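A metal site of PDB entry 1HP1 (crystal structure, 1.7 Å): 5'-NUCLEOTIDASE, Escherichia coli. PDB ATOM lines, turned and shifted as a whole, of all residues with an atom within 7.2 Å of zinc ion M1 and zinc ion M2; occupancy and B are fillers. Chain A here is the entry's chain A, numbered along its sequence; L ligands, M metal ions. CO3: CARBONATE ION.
The backbone NH of His 92 is in hydrogen-bond range of the side-chain carboxylate of Asp 59.
The backbone carbonyl oxygen (O) of Asp 16 is in hydrogen-bond range of the backbone NH (N) of Trp 266.
A ring nitrogen (ND1) of His 18 sits at hydrogen-bond distance from the backbone carbonyl oxygen of Asn 61 (2.9 Å).
The side-chain amide nitrogen (NE2) of Gln 229 sits at hydrogen-bond distance from the side-chain carboxylate (OE1) of Glu 265.
ND1 of His 18 is in hydrogen-bond range of O of Thr 62, 2.8 Å away.
O of His 192 sits at hydrogen-bond distance from N of Thr 147 (2.9 Å).
O of Gly 57 sits at hydrogen-bond distance from ND1 of His 192.
The backbone NH (N) of Asp 16 sits at hydrogen-bond distance from the backbone carbonyl oxygen (O) of Gly 58 (2.7 Å).
Of the 27 residues printed, 5 come within 4 Å of zinc ion M1.
Of the 27 residues printed, 4 come within 4 Å of zinc ion M2.
The nearest printed residue that does not touch zinc ion M2 is His 192 (4.2 Å).
Zinc ion M1 is bound by a ring nitrogen (NE2) of His 192 (2.1 Å), the side-chain amide oxygen of Asn 91 (2.1 Å), the side-chain carboxylate of Asp 59 (2.2 Å) and a ring nitrogen (ND1) of His 227 (2.3 Å).
Slightly farther from zinc ion M1 lies O1 of the ligand (2.7 Å).
Slightly farther from zinc ion M1 lies an oxygen (O3) of the ligand (2.8 Å).
OD2 of Asp 16 binds zinc ion M2 (2.1 Å).
Zinc ion M2 is bound by NE2 of His 18.
Zinc ion M2 is bound by the side-chain amide oxygen (OE1) of Gln 229, at 2.3 Å.
OD2 of Asp 59 is bound to zinc ion M2 (2.3 Å).
O1 of the ligand binds zinc ion M2 (2.6 Å).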
ATOM      1  N   ASN A  15     -35.686  21.834  19.244  1.00  0.00           N
ATOM      2  CA  ASN A  15     -34.797  22.872  18.713  1.00  0.00           C
ATOM      3  C   ASN A  15     -33.905  22.284  17.629  1.00  0.00           C
ATOM      4  O   ASN A  15     -33.722  21.073  17.553  1.00  0.00           O
ATOM      5  CB  ASN A  15     -33.899  23.429  19.833  1.00  0.00           C
ATOM      6  CG  ASN A  15     -33.086  22.337  20.521  1.00  0.00           C
ATOM      7  OD1 ASN A  15     -33.591  21.633  21.394  1.00  0.00           O
ATOM      8  ND2 ASN A  15     -31.830  22.164  20.098  1.00  0.00           N
ATOM      9  N   ASP A  16     -33.351  23.162  16.797  1.00  0.00           N
ATOM     10  CA  ASP A  16     -32.388  22.760  15.779  1.00  0.00           C
ATOM     11  C   ASP A  16     -32.900  21.623  14.915  1.00  0.00           C
ATOM     12  O   ASP A  16     -32.210  20.651  14.608  1.00  0.00           O
ATOM     13  CB  ASP A  16     -31.059  22.425  16.465  1.00  0.00           C
ATOM     14  CG  ASP A  16     -30.485  23.647  17.152  1.00  0.00           C
ATOM     15  OD1 ASP A  16     -30.840  23.937  18.288  1.00  0.00           O
ATOM     16  OD2 ASP A  16     -29.718  24.376  16.518  1.00  0.00           O
ATOM     17  N   HIS A  17     -34.134  21.808  14.480  1.00  0.00           N
ATOM     18  CA  HIS A  17     -34.838  20.879  13.614  1.00  0.00           C
ATOM     19  C   HIS A  17     -34.043  20.692  12.303  1.00  0.00           C
ATOM     20  O   HIS A  17     -33.953  19.590  11.776  1.00  0.00           O
ATOM     21  CB  HIS A  17     -36.212  21.482  13.373  1.00  0.00           C
ATOM     22  CG  HIS A  17     -37.028  20.742  12.374  1.00  0.00           C
ATOM     23  ND1 HIS A  17     -37.635  19.532  12.638  1.00  0.00           N
ATOM     24  CD2 HIS A  17     -37.307  21.034  11.076  1.00  0.00           C
ATOM     25  CE1 HIS A  17     -38.249  19.105  11.550  1.00  0.00           C
ATOM     26  NE2 HIS A  17     -38.074  20.002  10.586  1.00  0.00           N
ATOM     27  N   HIS A  18     -33.502  21.779  11.771  1.00  0.00           N
ATOM     28  CA  HIS A  18     -32.661  21.719  10.577  1.00  0.00           C
ATOM     29  C   HIS A  18     -33.144  20.900   9.412  1.00  0.00           C
ATOM     30  O   HIS A  18     -32.433  20.017   8.908  1.00  0.00           O
ATOM     31  CB  HIS A  18     -31.254  21.271  10.979  1.00  0.00           C
ATOM     32  CG  HIS A  18     -30.490  22.332  11.687  1.00  0.00           C
ATOM     33  ND1 HIS A  18     -30.243  23.566  11.110  1.00  0.00           N
ATOM     34  CD2 HIS A  18     -29.935  22.366  12.913  1.00  0.00           C
ATOM     35  CE1 HIS A  18     -29.557  24.310  11.961  1.00  0.00           C
ATOM     36  NE2 HIS A  18     -29.360  23.608  13.058  1.00  0.00           N
ATOM     37  N   GLY A  57     -36.617  26.114  19.975  1.00  0.00           N
ATOM     38  CA  GLY A  57     -35.417  26.908  20.156  1.00  0.00           C
ATOM     39  C   GLY A  57     -34.837  27.403  18.821  1.00  0.00           C
ATOM     40  O   GLY A  57     -33.737  27.948  18.790  1.00  0.00           O
ATOM     41  N   GLY A  58     -35.553  27.185  17.729  1.00  0.00           N
ATOM     42  CA  GLY A  58     -35.077  27.713  16.448  1.00  0.00           C
ATOM     43  C   GLY A  58     -34.170  26.849  15.610  1.00  0.00           C
ATOM     44  O   GLY A  58     -33.880  25.710  15.957  1.00  0.00           O
ATOM     45  N   ASP A  59     -33.688  27.414  14.506  1.00  0.00           N
ATOM     46  CA  ASP A  59     -32.859  26.699  13.531  1.00  0.00           C
ATOM     47  C   ASP A  59     -33.704  25.626  12.866  1.00  0.00           C
ATOM     48  O   ASP A  59     -33.401  24.427  12.906  1.00  0.00           O
ATOM     49  CB  ASP A  59     -31.572  26.109  14.141  1.00  0.00           C
ATOM     50  CG  ASP A  59     -30.393  27.040  13.984  1.00  0.00           C
ATOM     51  OD1 ASP A  59     -30.550  28.210  13.576  1.00  0.00           O
ATOM     52  OD2 ASP A  59     -29.263  26.609  14.288  1.00  0.00           O
ATOM     53  N   ILE A  60     -34.781  26.071  12.229  1.00  0.00           N
ATOM     54  CA  ILE A  60     -35.664  25.174  11.499  1.00  0.00           C
ATOM     55  C   ILE A  60     -35.015  24.977  10.145  1.00  0.00           C
ATOM     56  O   ILE A  60     -35.097  23.907   9.542  1.00  0.00           O
ATOM     57  CB  ILE A  60     -37.048  25.836  11.294  1.00  0.00           C
ATOM     58  CG1 ILE A  60     -37.616  26.240  12.653  1.00  0.00           C
ATOM     59  CG2 ILE A  60     -38.004  24.867  10.548  1.00  0.00           C
ATOM     60  CD1 ILE A  60     -37.587  25.108  13.692  1.00  0.00           C
ATOM     61  N   ASN A  61     -34.373  26.045   9.656  1.00  0.00           N
ATOM     62  CA  ASN A  61     -33.708  26.001   8.362  1.00  0.00           C
ATOM     63  C   ASN A  61     -32.376  25.285   8.336  1.00  0.00           C
ATOM     64  O   ASN A  61     -31.604  25.317   9.308  1.00  0.00           O
ATOM     65  CB  ASN A  61     -33.357  27.423   7.880  1.00  0.00           C
ATOM     66  CG  ASN A  61     -34.550  28.188   7.397  1.00  0.00           C
ATOM     67  OD1 ASN A  61     -34.892  28.137   6.221  1.00  0.00           O
ATOM     68  ND2 ASN A  61     -35.208  28.919   8.314  1.00  0.00           N
ATOM     69  N   THR A  62     -32.148  24.701   7.160  1.00  0.00           N
ATOM     70  CA  THR A  62     -30.888  24.149   6.717  1.00  0.00           C
ATOM     71  C   THR A  62     -30.355  22.866   7.256  1.00  0.00           C
ATOM     72  O   THR A  62     -30.022  22.786   8.430  1.00  0.00           O
ATOM     73  CB  THR A  62     -29.830  25.232   6.863  1.00  0.00           C
ATOM     74  OG1 THR A  62     -30.387  26.469   6.379  1.00  0.00           O
ATOM     75  CG2 THR A  62     -28.555  24.869   6.058  1.00  0.00           C
ATOM     76  N   GLY A  90     -33.377  31.384  15.087  1.00  0.00           N
ATOM     77  CA  GLY A  90     -32.022  30.860  15.166  1.00  0.00           C
ATOM     78  C   GLY A  90     -31.089  31.488  14.168  1.00  0.00           C
ATOM     79  O   GLY A  90     -31.539  32.182  13.243  1.00  0.00           O
ATOM     80  N   ASN A  91     -29.777  31.258  14.313  1.00  0.00           N
ATOM     81  CA  ASN A  91     -28.868  31.859  13.324  1.00  0.00           C
ATOM     82  C   ASN A  91     -29.090  31.335  11.919  1.00  0.00           C
ATOM     83  O   ASN A  91     -28.879  32.073  10.952  1.00  0.00           O
ATOM     84  CB  ASN A  91     -27.395  31.656  13.734  1.00  0.00           C
ATOM     85  CG  ASN A  91     -27.011  30.201  13.891  1.00  0.00           C
ATOM     86  OD1 ASN A  91     -27.676  29.457  14.577  1.00  0.00           O
ATOM     87  ND2 ASN A  91     -25.904  29.791  13.269  1.00  0.00           N
ATOM     88  N   HIS A  92     -29.517  30.072  11.765  1.00  0.00           N
ATOM     89  CA  HIS A  92     -29.730  29.588  10.406  1.00  0.00           C
ATOM     90  C   HIS A  92     -30.977  30.134   9.733  1.00  0.00           C
ATOM     91  O   HIS A  92     -31.188  29.938   8.554  1.00  0.00           O
ATOM     92  CB  HIS A  92     -29.691  28.050  10.406  1.00  0.00           C
ATOM     93  CG  HIS A  92     -28.306  27.500  10.543  1.00  0.00           C
ATOM     94  ND1 HIS A  92     -27.455  27.322   9.466  1.00  0.00           N
ATOM     95  CD2 HIS A  92     -27.603  27.144  11.640  1.00  0.00           C
ATOM     96  CE1 HIS A  92     -26.287  26.888   9.907  1.00  0.00           C
ATOM     97  NE2 HIS A  92     -26.348  26.766  11.211  1.00  0.00           N
ATOM     98  N   THR A 147     -28.542  34.125  19.298  1.00  0.00           N
ATOM     99  CA  THR A 147     -27.131  34.333  19.541  1.00  0.00           C
ATOM    100  C   THR A 147     -26.550  35.511  18.760  1.00  0.00           C
ATOM    101  O   THR A 147     -26.868  35.692  17.581  1.00  0.00           O
ATOM    102  CB  THR A 147     -26.291  33.076  19.219  1.00  0.00           C
ATOM    103  OG1 THR A 147     -24.914  33.415  19.400  1.00  0.00           O
ATOM    104  CG2 THR A 147     -26.511  32.573  17.790  1.00  0.00           C
ATOM    105  N   THR A 150     -24.508  35.311  15.333  1.00  0.00           N
ATOM    106  CA  THR A 150     -25.149  35.060  14.027  1.00  0.00           C
ATOM    107  C   THR A 150     -24.499  35.714  12.809  1.00  0.00           C
ATOM    108  O   THR A 150     -24.232  35.044  11.808  1.00  0.00           O
ATOM    109  CB  THR A 150     -26.657  35.458  14.081  1.00  0.00           C
ATOM    110  OG1 THR A 150     -27.319  34.617  15.049  1.00  0.00           O
ATOM    111  CG2 THR A 150     -27.356  35.251  12.722  1.00  0.00           C
ATOM    112  N   ILE A 153     -20.155  34.785  12.396  1.00  0.00           N
ATOM    113  CA  ILE A 153     -19.495  33.596  11.942  1.00  0.00           C
ATOM    114  C   ILE A 153     -19.508  33.282  10.474  1.00  0.00           C
ATOM    115  O   ILE A 153     -20.388  33.674   9.711  1.00  0.00           O
ATOM    116  CB  ILE A 153     -19.957  32.394  12.743  1.00  0.00           C
ATOM    117  CG1 ILE A 153     -21.463  32.251  12.628  1.00  0.00           C
ATOM    118  CG2 ILE A 153     -19.587  32.577  14.236  1.00  0.00           C
ATOM    119  CD1 ILE A 153     -22.039  31.261  13.696  1.00  0.00           C
ATOM    120  N   HIS A 192     -31.715  30.841  21.315  1.00  0.00           N
ATOM    121  CA  HIS A 192     -30.897  30.104  20.379  1.00  0.00           C
ATOM    122  C   HIS A 192     -29.511  30.594  20.691  1.00  0.00           C
ATOM    123  O   HIS A 192     -28.900  31.352  19.923  1.00  0.00           O
ATOM    124  CB  HIS A 192     -31.264  30.462  18.961  1.00  0.00           C
ATOM    125  CG  HIS A 192     -30.704  29.492  18.002  1.00  0.00           C
ATOM    126  ND1 HIS A 192     -31.270  28.262  17.801  1.00  0.00           N
ATOM    127  CD2 HIS A 192     -29.510  29.479  17.351  1.00  0.00           C
ATOM    128  CE1 HIS A 192     -30.462  27.513  17.073  1.00  0.00           C
ATOM    129  NE2 HIS A 192     -29.393  28.226  16.793  1.00  0.00           N
ATOM    130  N   MET A 193     -28.996  30.122  21.815  1.00  0.00           N
ATOM    131  CA  MET A 193     -27.740  30.671  22.335  1.00  0.00           C
ATOM    132  C   MET A 193     -26.684  29.639  22.704  1.00  0.00           C
ATOM    133  O   MET A 193     -25.492  29.958  22.724  1.00  0.00           O
ATOM    134  CB  MET A 193     -28.075  31.550  23.549  1.00  0.00           C
ATOM    135  CG  MET A 193     -28.790  32.853  23.144  1.00  0.00           C
ATOM    136  SD  MET A 193     -29.504  33.747  24.582  1.00  0.00           S
ATOM    137  CE  MET A 193     -28.068  33.852  25.658  1.00  0.00           C
ATOM    138  N   GLY A 226     -31.123  26.039  22.452  1.00  0.00           N
ATOM    139  CA  GLY A 226     -30.775  25.407  21.182  1.00  0.00           C
ATOM    140  C   GLY A 226     -29.371  25.816  20.811  1.00  0.00           C
ATOM    141  O   GLY A 226     -28.585  26.194  21.678  1.00  0.00           O
ATOM    142  N   HIS A 227     -29.086  25.738  19.510  1.00  0.00           N
ATOM    143  CA  HIS A 227     -27.807  26.146  18.924  1.00  0.00           C
ATOM    144  C   HIS A 227     -26.634  25.211  19.146  1.00  0.00           C
ATOM    145  O   HIS A 227     -26.030  24.755  18.168  1.00  0.00           O
ATOM    146  CB  HIS A 227     -27.438  27.584  19.370  1.00  0.00           C
ATOM    147  CG  HIS A 227     -26.276  28.164  18.603  1.00  0.00           C
ATOM    148  ND1 HIS A 227     -26.190  28.136  17.232  1.00  0.00           N
ATOM    149  CD2 HIS A 227     -25.157  28.788  19.027  1.00  0.00           C
ATOM    150  CE1 HIS A 227     -25.068  28.705  16.842  1.00  0.00           C
ATOM    151  NE2 HIS A 227     -24.418  29.107  17.915  1.00  0.00           N
ATOM    152  N   SER A 228     -26.316  24.920  20.415  1.00  0.00           N
ATOM    153  CA  SER A 228     -25.204  24.032  20.701  1.00  0.00           C
ATOM    154  C   SER A 228     -25.512  22.575  20.293  1.00  0.00           C
ATOM    155  O   SER A 228     -24.589  21.782  20.068  1.00  0.00           O
ATOM    156  CB  SER A 228     -24.787  24.131  22.179  1.00  0.00           C
ATOM    157  OG  SER A 228     -25.864  23.875  23.068  1.00  0.00           O
ATOM    158  N   GLN A 229     -26.799  22.277  20.156  1.00  0.00           N
ATOM    159  CA  GLN A 229     -27.317  20.981  19.741  1.00  0.00           C
ATOM    160  C   GLN A 229     -26.921  19.850  20.656  1.00  0.00           C
ATOM    161  O   GLN A 229     -26.144  18.946  20.284  1.00  0.00           O
ATOM    162  CB  GLN A 229     -26.930  20.698  18.279  1.00  0.00           C
ATOM    163  CG  GLN A 229     -27.635  21.720  17.381  1.00  0.00           C
ATOM    164  CD  GLN A 229     -27.474  21.497  15.881  1.00  0.00           C
ATOM    165  OE1 GLN A 229     -27.575  22.445  15.103  1.00  0.00           O
ATOM    166  NE2 GLN A 229     -27.286  20.259  15.456  1.00  0.00           N
ATOM    167  N   HIS A 264     -31.540  18.469  21.944  1.00  0.00           N
ATOM    168  CA  HIS A 264     -30.582  18.016  20.957  1.00  0.00           C
ATOM    169  C   HIS A 264     -30.781  18.611  19.571  1.00  0.00           C
ATOM    170  O   HIS A 264     -30.405  19.750  19.361  1.00  0.00           O
ATOM    171  CB  HIS A 264     -30.515  16.481  20.928  1.00  0.00           C
ATOM    172  CG  HIS A 264     -29.225  15.977  20.358  1.00  0.00           C
ATOM    173  ND1 HIS A 264     -28.840  14.644  20.407  1.00  0.00           N
ATOM    174  CD2 HIS A 264     -28.259  16.630  19.694  1.00  0.00           C
ATOM    175  CE1 HIS A 264     -27.682  14.513  19.786  1.00  0.00           C
ATOM    176  NE2 HIS A 264     -27.304  15.697  19.325  1.00  0.00           N
ATOM    177  N   GLU A 265     -31.387  17.894  18.645  1.00  0.00           N
ATOM    178  CA  GLU A 265     -31.535  18.416  17.284  1.00  0.00           C
ATOM    179  C   GLU A 265     -32.428  17.490  16.467  1.00  0.00           C
ATOM    180  O   GLU A 265     -32.743  16.395  16.912  1.00  0.00           O
ATOM    181  CB  GLU A 265     -30.150  18.398  16.620  1.00  0.00           C
ATOM    182  CG  GLU A 265     -29.653  16.938  16.482  1.00  0.00           C
ATOM    183  CD  GLU A 265     -28.183  16.784  16.205  1.00  0.00           C
ATOM    184  OE1 GLU A 265     -27.426  17.795  16.238  1.00  0.00           O
ATOM    185  OE2 GLU A 265     -27.779  15.627  15.969  1.00  0.00           O
ATOM    186  N   TRP A 266     -32.842  17.980  15.294  1.00  0.00           N
ATOM    187  CA  TRP A 266     -33.516  17.187  14.270  1.00  0.00           C
ATOM    188  C   TRP A 266     -34.800  16.489  14.633  1.00  0.00           C
ATOM    189  O   TRP A 266     -35.128  15.469  14.012  1.00  0.00           O
ATOM    190  CB  TRP A 266     -32.553  16.094  13.738  1.00  0.00           C
ATOM    191  CG  TRP A 266     -31.207  16.584  13.221  1.00  0.00           C
ATOM    192  CD1 TRP A 266     -30.781  17.886  13.094  1.00  0.00           C
ATOM    193  CD2 TRP A 266     -30.151  15.770  12.719  1.00  0.00           C
ATOM    194  NE1 TRP A 266     -29.515  17.916  12.524  1.00  0.00           N
ATOM    195  CE2 TRP A 266     -29.120  16.629  12.286  1.00  0.00           C
ATOM    196  CE3 TRP A 266     -29.986  14.389  12.594  1.00  0.00           C
ATOM    197  CZ2 TRP A 266     -27.926  16.159  11.733  1.00  0.00           C
ATOM    198  CZ3 TRP A 266     -28.793  13.914  12.033  1.00  0.00           C
ATOM    199  CH2 TRP A 266     -27.787  14.805  11.609  1.00  0.00           C
ATOM    200  N   THR A 484     -20.267  24.902  11.807  1.00  0.00           N
ATOM    201  CA  THR A 484     -21.242  25.779  11.143  1.00  0.00           C
ATOM    202  C   THR A 484     -22.625  25.194  10.946  1.00  0.00           C
ATOM    203  O   THR A 484     -23.572  25.965  10.670  1.00  0.00           O
ATOM    204  CB  THR A 484     -20.750  26.181   9.759  1.00  0.00           C
ATOM    205  OG1 THR A 484     -20.867  25.054   8.866  1.00  0.00           O
ATOM    206  CG2 THR A 484     -19.267  26.604   9.826  1.00  0.00           C
ATOM    207  N   GLY A 485     -22.759  23.889  11.044  1.00  0.00           N
ATOM    208  CA  GLY A 485     -24.060  23.254  10.818  1.00  0.00           C
ATOM    209  C   GLY A 485     -24.372  23.042   9.346  1.00  0.00           C
ATOM    210  O   GLY A 485     -25.426  22.488   8.988  1.00  0.00           O
HETATM  211  C   CO3 L   1     -25.512  26.010  14.151  1.00  0.00           C
HETATM  212  O1  CO3 L   1     -26.226  25.529  15.063  1.00  0.00           O
HETATM  213  O2  CO3 L   1     -24.767  25.322  13.396  1.00  0.00           O
HETATM  214  O3  CO3 L   1     -25.593  27.254  13.993  1.00  0.00           O
HETATM  215 ZN    ZN M   1     -27.786  27.647  15.621  1.00  0.00          ZN
HETATM  216 ZN    ZN M   2     -28.583  24.472  14.788  1.00  0.00          ZN
